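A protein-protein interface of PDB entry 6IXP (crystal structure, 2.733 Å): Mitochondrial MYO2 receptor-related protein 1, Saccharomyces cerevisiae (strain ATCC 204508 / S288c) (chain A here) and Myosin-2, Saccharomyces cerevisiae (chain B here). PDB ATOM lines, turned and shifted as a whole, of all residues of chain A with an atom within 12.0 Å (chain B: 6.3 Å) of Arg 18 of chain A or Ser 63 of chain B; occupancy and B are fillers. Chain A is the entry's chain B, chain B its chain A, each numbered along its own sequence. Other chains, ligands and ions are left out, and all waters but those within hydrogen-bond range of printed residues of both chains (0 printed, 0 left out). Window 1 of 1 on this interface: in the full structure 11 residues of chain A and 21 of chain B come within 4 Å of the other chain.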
ATOM      1  N   PRO A  13      -1.032 -31.839   4.133  1.00  0.00           N
ATOM      2  CA  PRO A  13      -2.048 -32.346   3.202  1.00  0.00           C
ATOM      3  C   PRO A  13      -2.896 -31.246   2.571  1.00  0.00           C
ATOM      4  O   PRO A  13      -2.966 -30.136   3.097  1.00  0.00           O
ATOM      5  CB  PRO A  13      -2.918 -33.246   4.089  1.00  0.00           C
ATOM      6  CG  PRO A  13      -2.053 -33.596   5.250  1.00  0.00           C
ATOM      7  CD  PRO A  13      -1.229 -32.373   5.491  1.00  0.00           C
ATOM      8  N   CYS A  14      -3.530 -31.565   1.447  1.00  0.00           N
ATOM      9  CA  CYS A  14      -4.462 -30.648   0.802  1.00  0.00           C
ATOM     10  C   CYS A  14      -5.690 -30.445   1.683  1.00  0.00           C
ATOM     11  O   CYS A  14      -6.175 -31.393   2.301  1.00  0.00           O
ATOM     12  CB  CYS A  14      -4.877 -31.180  -0.572  1.00  0.00           C
ATOM     13  SG  CYS A  14      -3.761 -30.739  -1.925  1.00  0.00           S
ATOM     14  N   PRO A  15      -6.194 -29.203   1.748  1.00  0.00           N
ATOM     15  CA  PRO A  15      -7.326 -28.877   2.621  1.00  0.00           C
ATOM     16  C   PRO A  15      -8.681 -29.227   2.002  1.00  0.00           C
ATOM     17  O   PRO A  15      -8.970 -28.845   0.868  1.00  0.00           O
ATOM     18  CB  PRO A  15      -7.186 -27.365   2.813  1.00  0.00           C
ATOM     19  CG  PRO A  15      -6.555 -26.895   1.548  1.00  0.00           C
ATOM     20  CD  PRO A  15      -5.643 -28.008   1.085  1.00  0.00           C
ATOM     21  N   LYS A  16      -9.498 -29.962   2.750  1.00  0.00           N
ATOM     22  CA  LYS A  16     -10.845 -30.307   2.311  1.00  0.00           C
ATOM     23  C   LYS A  16     -11.778 -29.117   2.496  1.00  0.00           C
ATOM     24  O   LYS A  16     -11.376 -28.080   3.022  1.00  0.00           O
ATOM     25  CB  LYS A  16     -11.381 -31.523   3.078  1.00  0.00           C
ATOM     26  CG  LYS A  16     -10.881 -32.875   2.579  1.00  0.00           C
ATOM     27  CD  LYS A  16      -9.412 -33.093   2.896  1.00  0.00           C
ATOM     28  CE  LYS A  16      -8.939 -34.449   2.414  1.00  0.00           C
ATOM     29  NZ  LYS A  16      -7.458 -34.573   2.494  1.00  0.00           N
ATOM     30  N   THR A  17     -13.023 -29.265   2.054  1.00  0.00           N
ATOM     31  CA  THR A  17     -14.022 -28.215   2.226  1.00  0.00           C
ATOM     32  C   THR A  17     -14.347 -27.998   3.706  1.00  0.00           C
ATOM     33  O   THR A  17     -14.607 -28.955   4.436  1.00  0.00           O
ATOM     34  CB  THR A  17     -15.320 -28.543   1.467  1.00  0.00           C
ATOM     35  OG1 THR A  17     -15.020 -28.796   0.090  1.00  0.00           O
ATOM     36  CG2 THR A  17     -16.305 -27.386   1.564  1.00  0.00           C
ATOM     37  N   ARG A  18     -14.328 -26.742   4.142  1.00  0.00           N
ATOM     38  CA  ARG A  18     -14.597 -26.425   5.541  1.00  0.00           C
ATOM     39  C   ARG A  18     -16.087 -26.564   5.857  1.00  0.00           C
ATOM     40  O   ARG A  18     -16.926 -25.875   5.270  1.00  0.00           O
ATOM     41  CB  ARG A  18     -14.113 -25.011   5.880  1.00  0.00           C
ATOM     42  CG  ARG A  18     -14.484 -24.564   7.285  1.00  0.00           C
ATOM     43  CD  ARG A  18     -14.053 -23.134   7.574  1.00  0.00           C
ATOM     44  NE  ARG A  18     -12.602 -22.985   7.614  1.00  0.00           N
ATOM     45  CZ  ARG A  18     -11.903 -22.245   6.759  1.00  0.00           C
ATOM     46  NH1 ARG A  18     -12.523 -21.579   5.795  1.00  0.00           N
ATOM     47  NH2 ARG A  18     -10.585 -22.168   6.873  1.00  0.00           N
ATOM     48  N   LEU A  19     -16.406 -27.454   6.793  1.00  0.00           N
ATOM     49  CA  LEU A  19     -17.793 -27.724   7.159  1.00  0.00           C
ATOM     50  C   LEU A  19     -18.481 -26.510   7.777  1.00  0.00           C
ATOM     51  O   LEU A  19     -19.522 -26.065   7.292  1.00  0.00           O
ATOM     52  CB  LEU A  19     -17.864 -28.911   8.120  1.00  0.00           C
ATOM     53  CG  LEU A  19     -17.819 -30.279   7.442  1.00  0.00           C
ATOM     54  CD1 LEU A  19     -17.548 -31.376   8.452  1.00  0.00           C
ATOM     55  CD2 LEU A  19     -19.123 -30.541   6.707  1.00  0.00           C
ATOM     56  N   ALA A  20     -17.893 -25.977   8.845  1.00  0.00           N
ATOM     57  CA  ALA A  20     -18.450 -24.811   9.519  1.00  0.00           C
ATOM     58  C   ALA A  20     -18.336 -23.566   8.649  1.00  0.00           C
ATOM     59  O   ALA A  20     -17.243 -23.192   8.229  1.00  0.00           O
ATOM     60  CB  ALA A  20     -17.755 -24.589  10.849  1.00  0.00           C
ATOM     61  N   ARG A  21     -19.469 -22.923   8.388  1.00  0.00           N
ATOM     62  CA  ARG A  21     -19.478 -21.710   7.578  1.00  0.00           C
ATOM     63  C   ARG A  21     -19.162 -20.495   8.446  1.00  0.00           C
ATOM     64  O   ARG A  21     -20.055 -19.792   8.917  1.00  0.00           O
ATOM     65  CB  ARG A  21     -20.821 -21.548   6.859  1.00  0.00           C
ATOM     66  CG  ARG A  21     -21.029 -22.572   5.739  1.00  0.00           C
ATOM     67  CD  ARG A  21     -22.313 -22.325   4.954  1.00  0.00           C
ATOM     68  NE  ARG A  21     -23.509 -22.755   5.673  1.00  0.00           N
ATOM     69  CZ  ARG A  21     -24.115 -23.924   5.486  1.00  0.00           C
ATOM     70  NH1 ARG A  21     -23.641 -24.784   4.594  1.00  0.00           N
ATOM     71  NH2 ARG A  21     -25.201 -24.232   6.184  1.00  0.00           N
ATOM     72  N   VAL A  22     -17.865 -20.273   8.646  1.00  0.00           N
ATOM     73  CA  VAL A  22     -17.350 -19.252   9.551  1.00  0.00           C
ATOM     74  C   VAL A  22     -17.697 -17.835   9.112  1.00  0.00           C
ATOM     75  O   VAL A  22     -17.409 -17.435   7.983  1.00  0.00           O
ATOM     76  CB  VAL A  22     -15.816 -19.364   9.679  1.00  0.00           C
ATOM     77  CG1 VAL A  22     -15.271 -18.287  10.610  1.00  0.00           C
ATOM     78  CG2 VAL A  22     -15.423 -20.753  10.159  1.00  0.00           C
ATOM     79  N   SER A  23     -18.309 -17.077  10.020  1.00  0.00           N
ATOM     80  CA  SER A  23     -18.707 -15.703   9.732  1.00  0.00           C
ATOM     81  C   SER A  23     -17.762 -14.691  10.385  1.00  0.00           C
ATOM     82  O   SER A  23     -17.272 -14.904  11.494  1.00  0.00           O
ATOM     83  CB  SER A  23     -20.142 -15.457  10.200  1.00  0.00           C
ATOM     84  OG  SER A  23     -20.586 -14.163   9.829  1.00  0.00           O
ATOM     85  N   VAL A  24     -17.508 -13.591   9.680  1.00  0.00           N
ATOM     86  CA  VAL A  24     -16.599 -12.552  10.157  1.00  0.00           C
ATOM     87  C   VAL A  24     -17.229 -11.734  11.283  1.00  0.00           C
ATOM     88  O   VAL A  24     -18.445 -11.758  11.471  1.00  0.00           O
ATOM     89  CB  VAL A  24     -16.180 -11.606   9.011  1.00  0.00           C
ATOM     90  CG1 VAL A  24     -15.563 -12.398   7.868  1.00  0.00           C
ATOM     91  CG2 VAL A  24     -17.374 -10.803   8.523  1.00  0.00           C
ATOM     92  N   ASN B  10      -2.523 -22.102   6.268  1.00  0.00           N
ATOM     93  CA  ASN B  10      -2.863 -23.520   6.334  1.00  0.00           C
ATOM     94  C   ASN B  10      -1.773 -24.327   7.039  1.00  0.00           C
ATOM     95  O   ASN B  10      -2.061 -25.296   7.750  1.00  0.00           O
ATOM     96  CB  ASN B  10      -3.105 -24.078   4.931  1.00  0.00           C
ATOM     97  CG  ASN B  10      -4.387 -23.558   4.310  1.00  0.00           C
ATOM     98  OD1 ASN B  10      -5.120 -22.788   4.927  1.00  0.00           O
ATOM     99  ND2 ASN B  10      -4.667 -23.984   3.083  1.00  0.00           N
ATOM    100  N   LEU B  13      -1.842 -23.461  10.785  1.00  0.00           N
ATOM    101  CA  LEU B  13      -3.078 -24.105  11.218  1.00  0.00           C
ATOM    102  C   LEU B  13      -2.869 -25.593  11.443  1.00  0.00           C
ATOM    103  O   LEU B  13      -3.309 -26.136  12.454  1.00  0.00           O
ATOM    104  CB  LEU B  13      -4.198 -23.891  10.201  1.00  0.00           C
ATOM    105  CG  LEU B  13      -5.054 -22.634  10.358  1.00  0.00           C
ATOM    106  CD1 LEU B  13      -6.097 -22.564   9.254  1.00  0.00           C
ATOM    107  CD2 LEU B  13      -5.713 -22.598  11.731  1.00  0.00           C
ATOM    108  N   LEU B  58     -15.339 -24.645  20.028  1.00  0.00           N
ATOM    109  CA  LEU B  58     -15.125 -26.076  19.820  1.00  0.00           C
ATOM    110  C   LEU B  58     -15.490 -26.504  18.403  1.00  0.00           C
ATOM    111  O   LEU B  58     -14.844 -27.374  17.822  1.00  0.00           O
ATOM    112  CB  LEU B  58     -15.940 -26.897  20.822  1.00  0.00           C
ATOM    113  CG  LEU B  58     -15.508 -26.857  22.289  1.00  0.00           C
ATOM    114  CD1 LEU B  58     -16.404 -27.745  23.141  1.00  0.00           C
ATOM    115  CD2 LEU B  58     -14.054 -27.254  22.433  1.00  0.00           C
ATOM    116  N   ILE B  59     -16.533 -25.883  17.859  1.00  0.00           N
ATOM    117  CA  ILE B  59     -17.021 -26.194  16.523  1.00  0.00           C
ATOM    118  C   ILE B  59     -16.022 -25.724  15.477  1.00  0.00           C
ATOM    119  O   ILE B  59     -15.732 -26.444  14.525  1.00  0.00           O
ATOM    120  CB  ILE B  59     -18.403 -25.553  16.261  1.00  0.00           C
ATOM    121  CG1 ILE B  59     -19.506 -26.386  16.920  1.00  0.00           C
ATOM    122  CG2 ILE B  59     -18.677 -25.439  14.769  1.00  0.00           C
ATOM    123  CD1 ILE B  59     -20.798 -25.623  17.158  1.00  0.00           C
ATOM    124  N   ILE B  60     -15.479 -24.525  15.662  1.00  0.00           N
ATOM    125  CA  ILE B  60     -14.485 -24.023  14.722  1.00  0.00           C
ATOM    126  C   ILE B  60     -13.237 -24.908  14.746  1.00  0.00           C
ATOM    127  O   ILE B  60     -12.731 -25.319  13.686  1.00  0.00           O
ATOM    128  CB  ILE B  60     -14.103 -22.560  15.026  1.00  0.00           C
ATOM    129  CG1 ILE B  60     -15.231 -21.628  14.588  1.00  0.00           C
ATOM    130  CG2 ILE B  60     -12.827 -22.176  14.302  1.00  0.00           C
ATOM    131  CD1 ILE B  60     -15.031 -20.189  14.989  1.00  0.00           C
ATOM    132  N   VAL B  61     -12.761 -25.231  15.949  1.00  0.00           N
ATOM    133  CA  VAL B  61     -11.588 -26.099  16.070  1.00  0.00           C
ATOM    134  C   VAL B  61     -11.820 -27.481  15.450  1.00  0.00           C
ATOM    135  O   VAL B  61     -10.970 -27.996  14.724  1.00  0.00           O
ATOM    136  CB  VAL B  61     -11.170 -26.282  17.535  1.00  0.00           C
ATOM    137  CG1 VAL B  61      -9.995 -27.247  17.629  1.00  0.00           C
ATOM    138  CG2 VAL B  61     -10.808 -24.940  18.151  1.00  0.00           C
ATOM    139  N   LEU B  62     -12.976 -28.072  15.734  1.00  0.00           N
ATOM    140  CA  LEU B  62     -13.318 -29.400  15.227  1.00  0.00           C
ATOM    141  C   LEU B  62     -13.436 -29.430  13.707  1.00  0.00           C
ATOM    142  O   LEU B  62     -12.891 -30.316  13.042  1.00  0.00           O
ATOM    143  CB  LEU B  62     -14.632 -29.879  15.848  1.00  0.00           C
ATOM    144  CG  LEU B  62     -15.098 -31.265  15.412  1.00  0.00           C
ATOM    145  CD1 LEU B  62     -14.093 -32.297  15.860  1.00  0.00           C
ATOM    146  CD2 LEU B  62     -16.469 -31.571  15.973  1.00  0.00           C
ATOM    147  N   SER B  63     -14.157 -28.452  13.169  1.00  0.00           N
ATOM    148  CA  SER B  63     -14.359 -28.330  11.735  1.00  0.00           C
ATOM    149  C   SER B  63     -13.029 -28.095  11.026  1.00  0.00           C
ATOM    150  O   SER B  63     -12.811 -28.583   9.910  1.00  0.00           O
ATOM    151  CB  SER B  63     -15.344 -27.197  11.439  1.00  0.00           C
ATOM    152  OG  SER B  63     -15.139 -26.637  10.156  1.00  0.00           O
ATOM    153  N   GLU B  64     -12.123 -27.377  11.682  1.00  0.00           N
ATOM    154  CA  GLU B  64     -10.818 -27.152  11.080  1.00  0.00           C
ATOM    155  C   GLU B  64      -9.952 -28.409  11.166  1.00  0.00           C
ATOM    156  O   GLU B  64      -9.131 -28.661  10.284  1.00  0.00           O
ATOM    157  CB  GLU B  64     -10.110 -25.965  11.733  1.00  0.00           C
ATOM    158  CG  GLU B  64      -9.016 -25.363  10.860  1.00  0.00           C
ATOM    159  CD  GLU B  64      -9.556 -24.674   9.611  1.00  0.00           C
ATOM    160  OE1 GLU B  64     -10.785 -24.479   9.502  1.00  0.00           O
ATOM    161  OE2 GLU B  64      -8.742 -24.342   8.724  1.00  0.00           O
ATOM    162  N   MET B  65     -10.138 -29.200  12.219  1.00  0.00           N
ATOM    163  CA  MET B  65      -9.494 -30.507  12.299  1.00  0.00           C
ATOM    164  C   MET B  65      -9.944 -31.398  11.146  1.00  0.00           C
ATOM    165  O   MET B  65      -9.125 -32.010  10.459  1.00  0.00           O
ATOM    166  CB  MET B  65      -9.801 -31.192  13.632  1.00  0.00           C
ATOM    167  CG  MET B  65      -9.017 -30.656  14.813  1.00  0.00           C
ATOM    168  SD  MET B  65      -9.299 -31.626  16.307  1.00  0.00           S
ATOM    169  CE  MET B  65      -8.272 -30.744  17.480  1.00  0.00           C
ATOM    170  N   TRP B  66     -11.256 -31.456  10.936  1.00  0.00           N
ATOM    171  CA  TRP B  66     -11.833 -32.262   9.867  1.00  0.00           C
ATOM    172  C   TRP B  66     -11.429 -31.734   8.491  1.00  0.00           C
ATOM    173  O   TRP B  66     -11.405 -32.483   7.514  1.00  0.00           O
ATOM    174  CB  TRP B  66     -13.359 -32.295   9.996  1.00  0.00           C
ATOM    175  CG  TRP B  66     -13.848 -33.207  11.087  1.00  0.00           C
ATOM    176  CD1 TRP B  66     -13.145 -34.207  11.696  1.00  0.00           C
ATOM    177  CD2 TRP B  66     -15.138 -33.187  11.711  1.00  0.00           C
ATOM    178  NE1 TRP B  66     -13.920 -34.817  12.651  1.00  0.00           N
ATOM    179  CE2 TRP B  66     -15.149 -34.210  12.681  1.00  0.00           C
ATOM    180  CE3 TRP B  66     -16.286 -32.407  11.542  1.00  0.00           C
ATOM    181  CZ2 TRP B  66     -16.262 -34.474  13.479  1.00  0.00           C
ATOM    182  CZ3 TRP B  66     -17.390 -32.670  12.335  1.00  0.00           C
ATOM    183  CH2 TRP B  66     -17.370 -33.695  13.290  1.00  0.00           C
ATOM    184  N   ARG B  67     -11.116 -30.442   8.423  1.00  0.00           N
ATOM    185  CA  ARG B  67     -10.639 -29.834   7.185  1.00  0.00           C
ATOM    186  C   ARG B  67      -9.316 -30.460   6.736  1.00  0.00           C
ATOM    187  O   ARG B  67      -9.108 -30.715   5.548  1.00  0.00           O
ATOM    188  CB  ARG B  67     -10.466 -28.323   7.364  1.00  0.00           C
ATOM    189  CG  ARG B  67     -10.337 -27.549   6.062  1.00  0.00           C
ATOM    190  CD  ARG B  67      -9.723 -26.174   6.290  1.00  0.00           C
ATOM    191  NE  ARG B  67      -9.585 -25.417   5.048  1.00  0.00           N
ATOM    192  CZ  ARG B  67      -8.685 -24.456   4.851  1.00  0.00           C
ATOM    193  NH1 ARG B  67      -7.826 -24.138   5.811  1.00  0.00           N
ATOM    194  NH2 ARG B  67      -8.632 -23.820   3.687  1.00  0.00           N
ATOM    195  N   PHE B  68      -8.431 -30.709   7.696  1.00  0.00           N
ATOM    196  CA  PHE B  68      -7.132 -31.310   7.413  1.00  0.00           C
ATOM    197  C   PHE B  68      -7.099 -32.807   7.716  1.00  0.00           C
ATOM    198  O   PHE B  68      -6.039 -33.364   7.995  1.00  0.00           O
ATOM    199  CB  PHE B  68      -6.042 -30.590   8.211  1.00  0.00           C
ATOM    200  CG  PHE B  68      -5.854 -29.153   7.815  1.00  0.00           C
ATOM    201  CD1 PHE B  68      -5.180 -28.823   6.647  1.00  0.00           C
ATOM    202  CD2 PHE B  68      -6.362 -28.130   8.601  1.00  0.00           C
ATOM    203  CE1 PHE B  68      -5.005 -27.503   6.276  1.00  0.00           C
ATOM    204  CE2 PHE B  68      -6.195 -26.806   8.238  1.00  0.00           C
ATOM    205  CZ  PHE B  68      -5.513 -26.493   7.071  1.00  0.00           C
ATOM    206  N   PHE B 114     -24.641 -29.191  15.656  1.00  0.00           N
ATOM    207  CA  PHE B 114     -23.627 -29.079  14.621  1.00  0.00           C
ATOM    208  C   PHE B 114     -23.203 -30.451  14.119  1.00  0.00           C
ATOM    209  O   PHE B 114     -23.109 -30.665  12.910  1.00  0.00           O
ATOM    210  CB  PHE B 114     -22.400 -28.322  15.121  1.00  0.00           C
ATOM    211  CG  PHE B 114     -21.266 -28.325  14.141  1.00  0.00           C
ATOM    212  CD1 PHE B 114     -21.324 -27.544  12.997  1.00  0.00           C
ATOM    213  CD2 PHE B 114     -20.161 -29.137  14.337  1.00  0.00           C
ATOM    214  CE1 PHE B 114     -20.292 -27.555  12.081  1.00  0.00           C
ATOM    215  CE2 PHE B 114     -19.131 -29.152  13.425  1.00  0.00           C
ATOM    216  CZ  PHE B 114     -19.196 -28.360  12.296  1.00  0.00           C
ATOM    217  N   PHE B 128     -17.616 -33.961  -0.457  1.00  0.00           N
ATOM    218  CA  PHE B 128     -16.834 -34.359   0.711  1.00  0.00           C
ATOM    219  C   PHE B 128     -16.132 -35.706   0.530  1.00  0.00           C
ATOM    220  O   PHE B 128     -15.568 -36.250   1.478  1.00  0.00           O
ATOM    221  CB  PHE B 128     -17.724 -34.396   1.953  1.00  0.00           C
ATOM    222  CG  PHE B 128     -18.241 -33.047   2.362  1.00  0.00           C
ATOM    223  CD1 PHE B 128     -17.387 -32.099   2.904  1.00  0.00           C
ATOM    224  CD2 PHE B 128     -19.579 -32.724   2.204  1.00  0.00           C
ATOM    225  CE1 PHE B 128     -17.858 -30.854   3.281  1.00  0.00           C
ATOM    226  CE2 PHE B 128     -20.058 -31.480   2.581  1.00  0.00           C
ATOM    227  CZ  PHE B 128     -19.196 -30.545   3.119  1.00  0.00           C
ATOM    228  N   LEU B 411      -6.477 -17.330  12.686  1.00  0.00           N
ATOM    229  CA  LEU B 411      -6.004 -17.750  11.365  1.00  0.00           C
ATOM    230  C   LEU B 411      -7.175 -18.078  10.437  1.00  0.00           C
ATOM    231  O   LEU B 411      -7.229 -17.603   9.291  1.00  0.00           O
ATOM    232  CB  LEU B 411      -5.072 -18.956  11.478  1.00  0.00           C
ATOM    233  CG  LEU B 411      -3.671 -18.703  12.034  1.00  0.00           C
ATOM    234  CD1 LEU B 411      -2.924 -20.012  12.212  1.00  0.00           C
ATOM    235  CD2 LEU B 411      -2.907 -17.772  11.113  1.00  0.00           C
ATOM    236  N   VAL B 412      -8.101 -18.896  10.936  1.00  0.00           N
ATOM    237  CA  VAL B 412      -9.298 -19.241  10.177  1.00  0.00           C
ATOM    238  C   VAL B 412     -10.065 -17.984   9.765  1.00  0.00           C
ATOM    239  O   VAL B 412     -10.507 -17.857   8.622  1.00  0.00           O
ATOM    240  CB  VAL B 412     -10.222 -20.174  10.980  1.00  0.00           C
ATOM    241  CG1 VAL B 412     -11.522 -20.423  10.227  1.00  0.00           C
ATOM    242  CG2 VAL B 412      -9.514 -21.488  11.280  1.00  0.00           C
ATOM    243  N   GLN B 415      -8.403 -16.263   6.962  1.00  0.00           N
ATOM    244  CA  GLN B 415      -8.655 -17.017   5.743  1.00  0.00           C
ATOM    245  C   GLN B 415     -10.044 -16.730   5.173  1.00  0.00           C
ATOM    246  O   GLN B 415     -10.208 -16.639   3.956  1.00  0.00           O
ATOM    247  CB  GLN B 415      -8.486 -18.511   6.010  1.00  0.00           C
ATOM    248  CG  GLN B 415      -8.259 -19.338   4.765  1.00  0.00           C
ATOM    249  CD  GLN B 415      -7.533 -20.629   5.065  1.00  0.00           C
ATOM    250  OE1 GLN B 415      -8.002 -21.455   5.846  1.00  0.00           O
ATOM    251  NE2 GLN B 415      -6.370 -20.808   4.449  1.00  0.00           N
ATOM    252  N   VAL B 416     -11.041 -16.597   6.044  1.00  0.00           N
ATOM    253  CA  VAL B 416     -12.386 -16.230   5.599  1.00  0.00           C
ATOM    254  C   VAL B 416     -12.450 -14.780   5.105  1.00  0.00           C
ATOM    255  O   VAL B 416     -13.153 -14.476   4.140  1.00  0.00           O
ATOM    256  CB  VAL B 416     -13.435 -16.430   6.715  1.00  0.00           C
ATOM    257  CG1 VAL B 416     -14.835 -16.185   6.174  1.00  0.00           C
ATOM    258  CG2 VAL B 416     -13.331 -17.827   7.296  1.00  0.00           C
ATOM    259  N   ASP B 419     -11.071 -14.744   1.457  1.00  0.00           N
ATOM    260  CA  ASP B 419     -12.103 -15.233   0.546  1.00  0.00           C
ATOM    261  C   ASP B 419     -13.372 -14.384   0.607  1.00  0.00           C
ATOM    262  O   ASP B 419     -13.358 -13.192   0.300  1.00  0.00           O
ATOM    263  CB  ASP B 419     -12.444 -16.693   0.857  1.00  0.00           C
ATOM    264  CG  ASP B 419     -11.323 -17.644   0.492  1.00  0.00           C
ATOM    265  OD1 ASP B 419     -10.401 -17.225  -0.238  1.00  0.00           O
ATOM    266  OD2 ASP B 419     -11.367 -18.813   0.931  1.00  0.00           O
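Of the 12 printed residues of chain A, 7 touch a printed residue of chain B.
Of the 20 printed residues of chain B, 9 touch a printed residue of chain A.
Hydrophobic or aromatic side chains of chain B within 4 Å of the printed part of chain A: Trp 66, Phe 128, Val 412 and Val 416.
Of chain B, only Ser 63, Glu 64, Arg 67, Val 412 and Gln 415 come within 4 Å of Arg 18 of chain A.
Ser 63 of chain B touches three residues of chain A.
No residue of chain A comes within 4 Å of Ile 60 of chain B.
Val 61 of chain B touches none of the printed residues of chain A.
No residue of chain A comes within 4 Å of Leu 62 of chain B.
Of chain A, only Arg 18 (3.0 Å) comes within 4 Å of Glu 64 of chain B.
No residue of chain A comes within 4 Å of Met 65 of chain B.
Of the printed residues of chain A, Arg 67 of chain B touches Pro 15, Lys 16 and Arg 18.
Val 412 of chain B touches just these residues of chain A: Arg 18 and Val 22.
Of chain A, only Arg 18 comes within 4 Å of Gln 415 of chain B.
Of the printed residues of chain B, Leu 19 of chain A touches Ser 63, Trp 66 and Phe 128.
Printed residues of chain B within 4 Å of Thr 17 of chain A: Phe 128 (3.9 Å).
Of the printed residues of chain B, Lys 16 of chain A touches Arg 67 (2.9 Å).
The nearest residue of chain B that does not touch Arg 18 of chain A is Val 416 of chain B (4.1 Å).
The nearest residue of chain A that does not touch Ser 63 of chain B is Thr 17 of chain A (5.8 Å).
The side-chain carboxylate of Glu 64 of chain B is in salt-bridge range of the guanidinium group of Arg 67 of chain B (3.1 Å).
O of Cys 14 of chain A sits at hydrogen-bond distance from NZ of Lys 16 of chain A, at 3.4 Å.
The guanidinium group of Arg 67 of chain B lies within hydrogen-bond range of the side-chain amide oxygen of Gln 415 of chain B, 2.7 Å away.
The side-chain amide oxygen (OD1) of Asn 10 of chain B lies close to the side-chain amide oxygen (OE1) of Gln 415 of chain B (3.3 Å).
NH1 of Arg 67 of chain B lies within hydrogen-bond range of OD1 of Asn 10 of chain B (3.2 Å).
Among the printed residues, merely in contact across the chains: Val 22 of chain A with Val 416 of chain B (3.4 Å), Leu 19 of chain A with Trp 66 of chain B (3.5 Å), Arg 18 of chain A with Arg 67 of chain B (3.6 Å), Leu 19 of chain A with Phe 128 of chain B (3.6 Å), Arg 18 of chain A with Ser 63 of chain B (3.6 Å), Leu 19 of chain A with Ser 63 of chain B (3.7 Å), Pro 15 of chain A with Asn 10 of chain B (3.8 Å), Pro 15 of chain A with Arg 67 of chain B (3.8 Å), Arg 18 of chain A with Val 412 of chain B (3.8 Å), Thr 17 of chain A with Phe 128 of chain B (3.9 Å) and Val 22 of chain A with Val 412 of chain B (3.9 Å).
The side-chain hydroxyl (OG) of Ser 63 of chain B is in hydrogen-bond range of the backbone NH (N) of Ala 20 of chain A (3.1 Å).
O of Arg 67 of chain B is in hydrogen-bond range of N of Lys 16 of chain A (2.9 Å).
The side-chain amide oxygen (OE1) of Gln 415 of chain B is in hydrogen-bond range of the guanidinium group (NH2) of Arg 18 of chain A (2.9 Å).
The side-chain carboxylate (OE1) of Glu 64 of chain B is in salt-bridge range of the guanidinium group (NE) of Arg 18 of chain A, 3.0 Å away.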
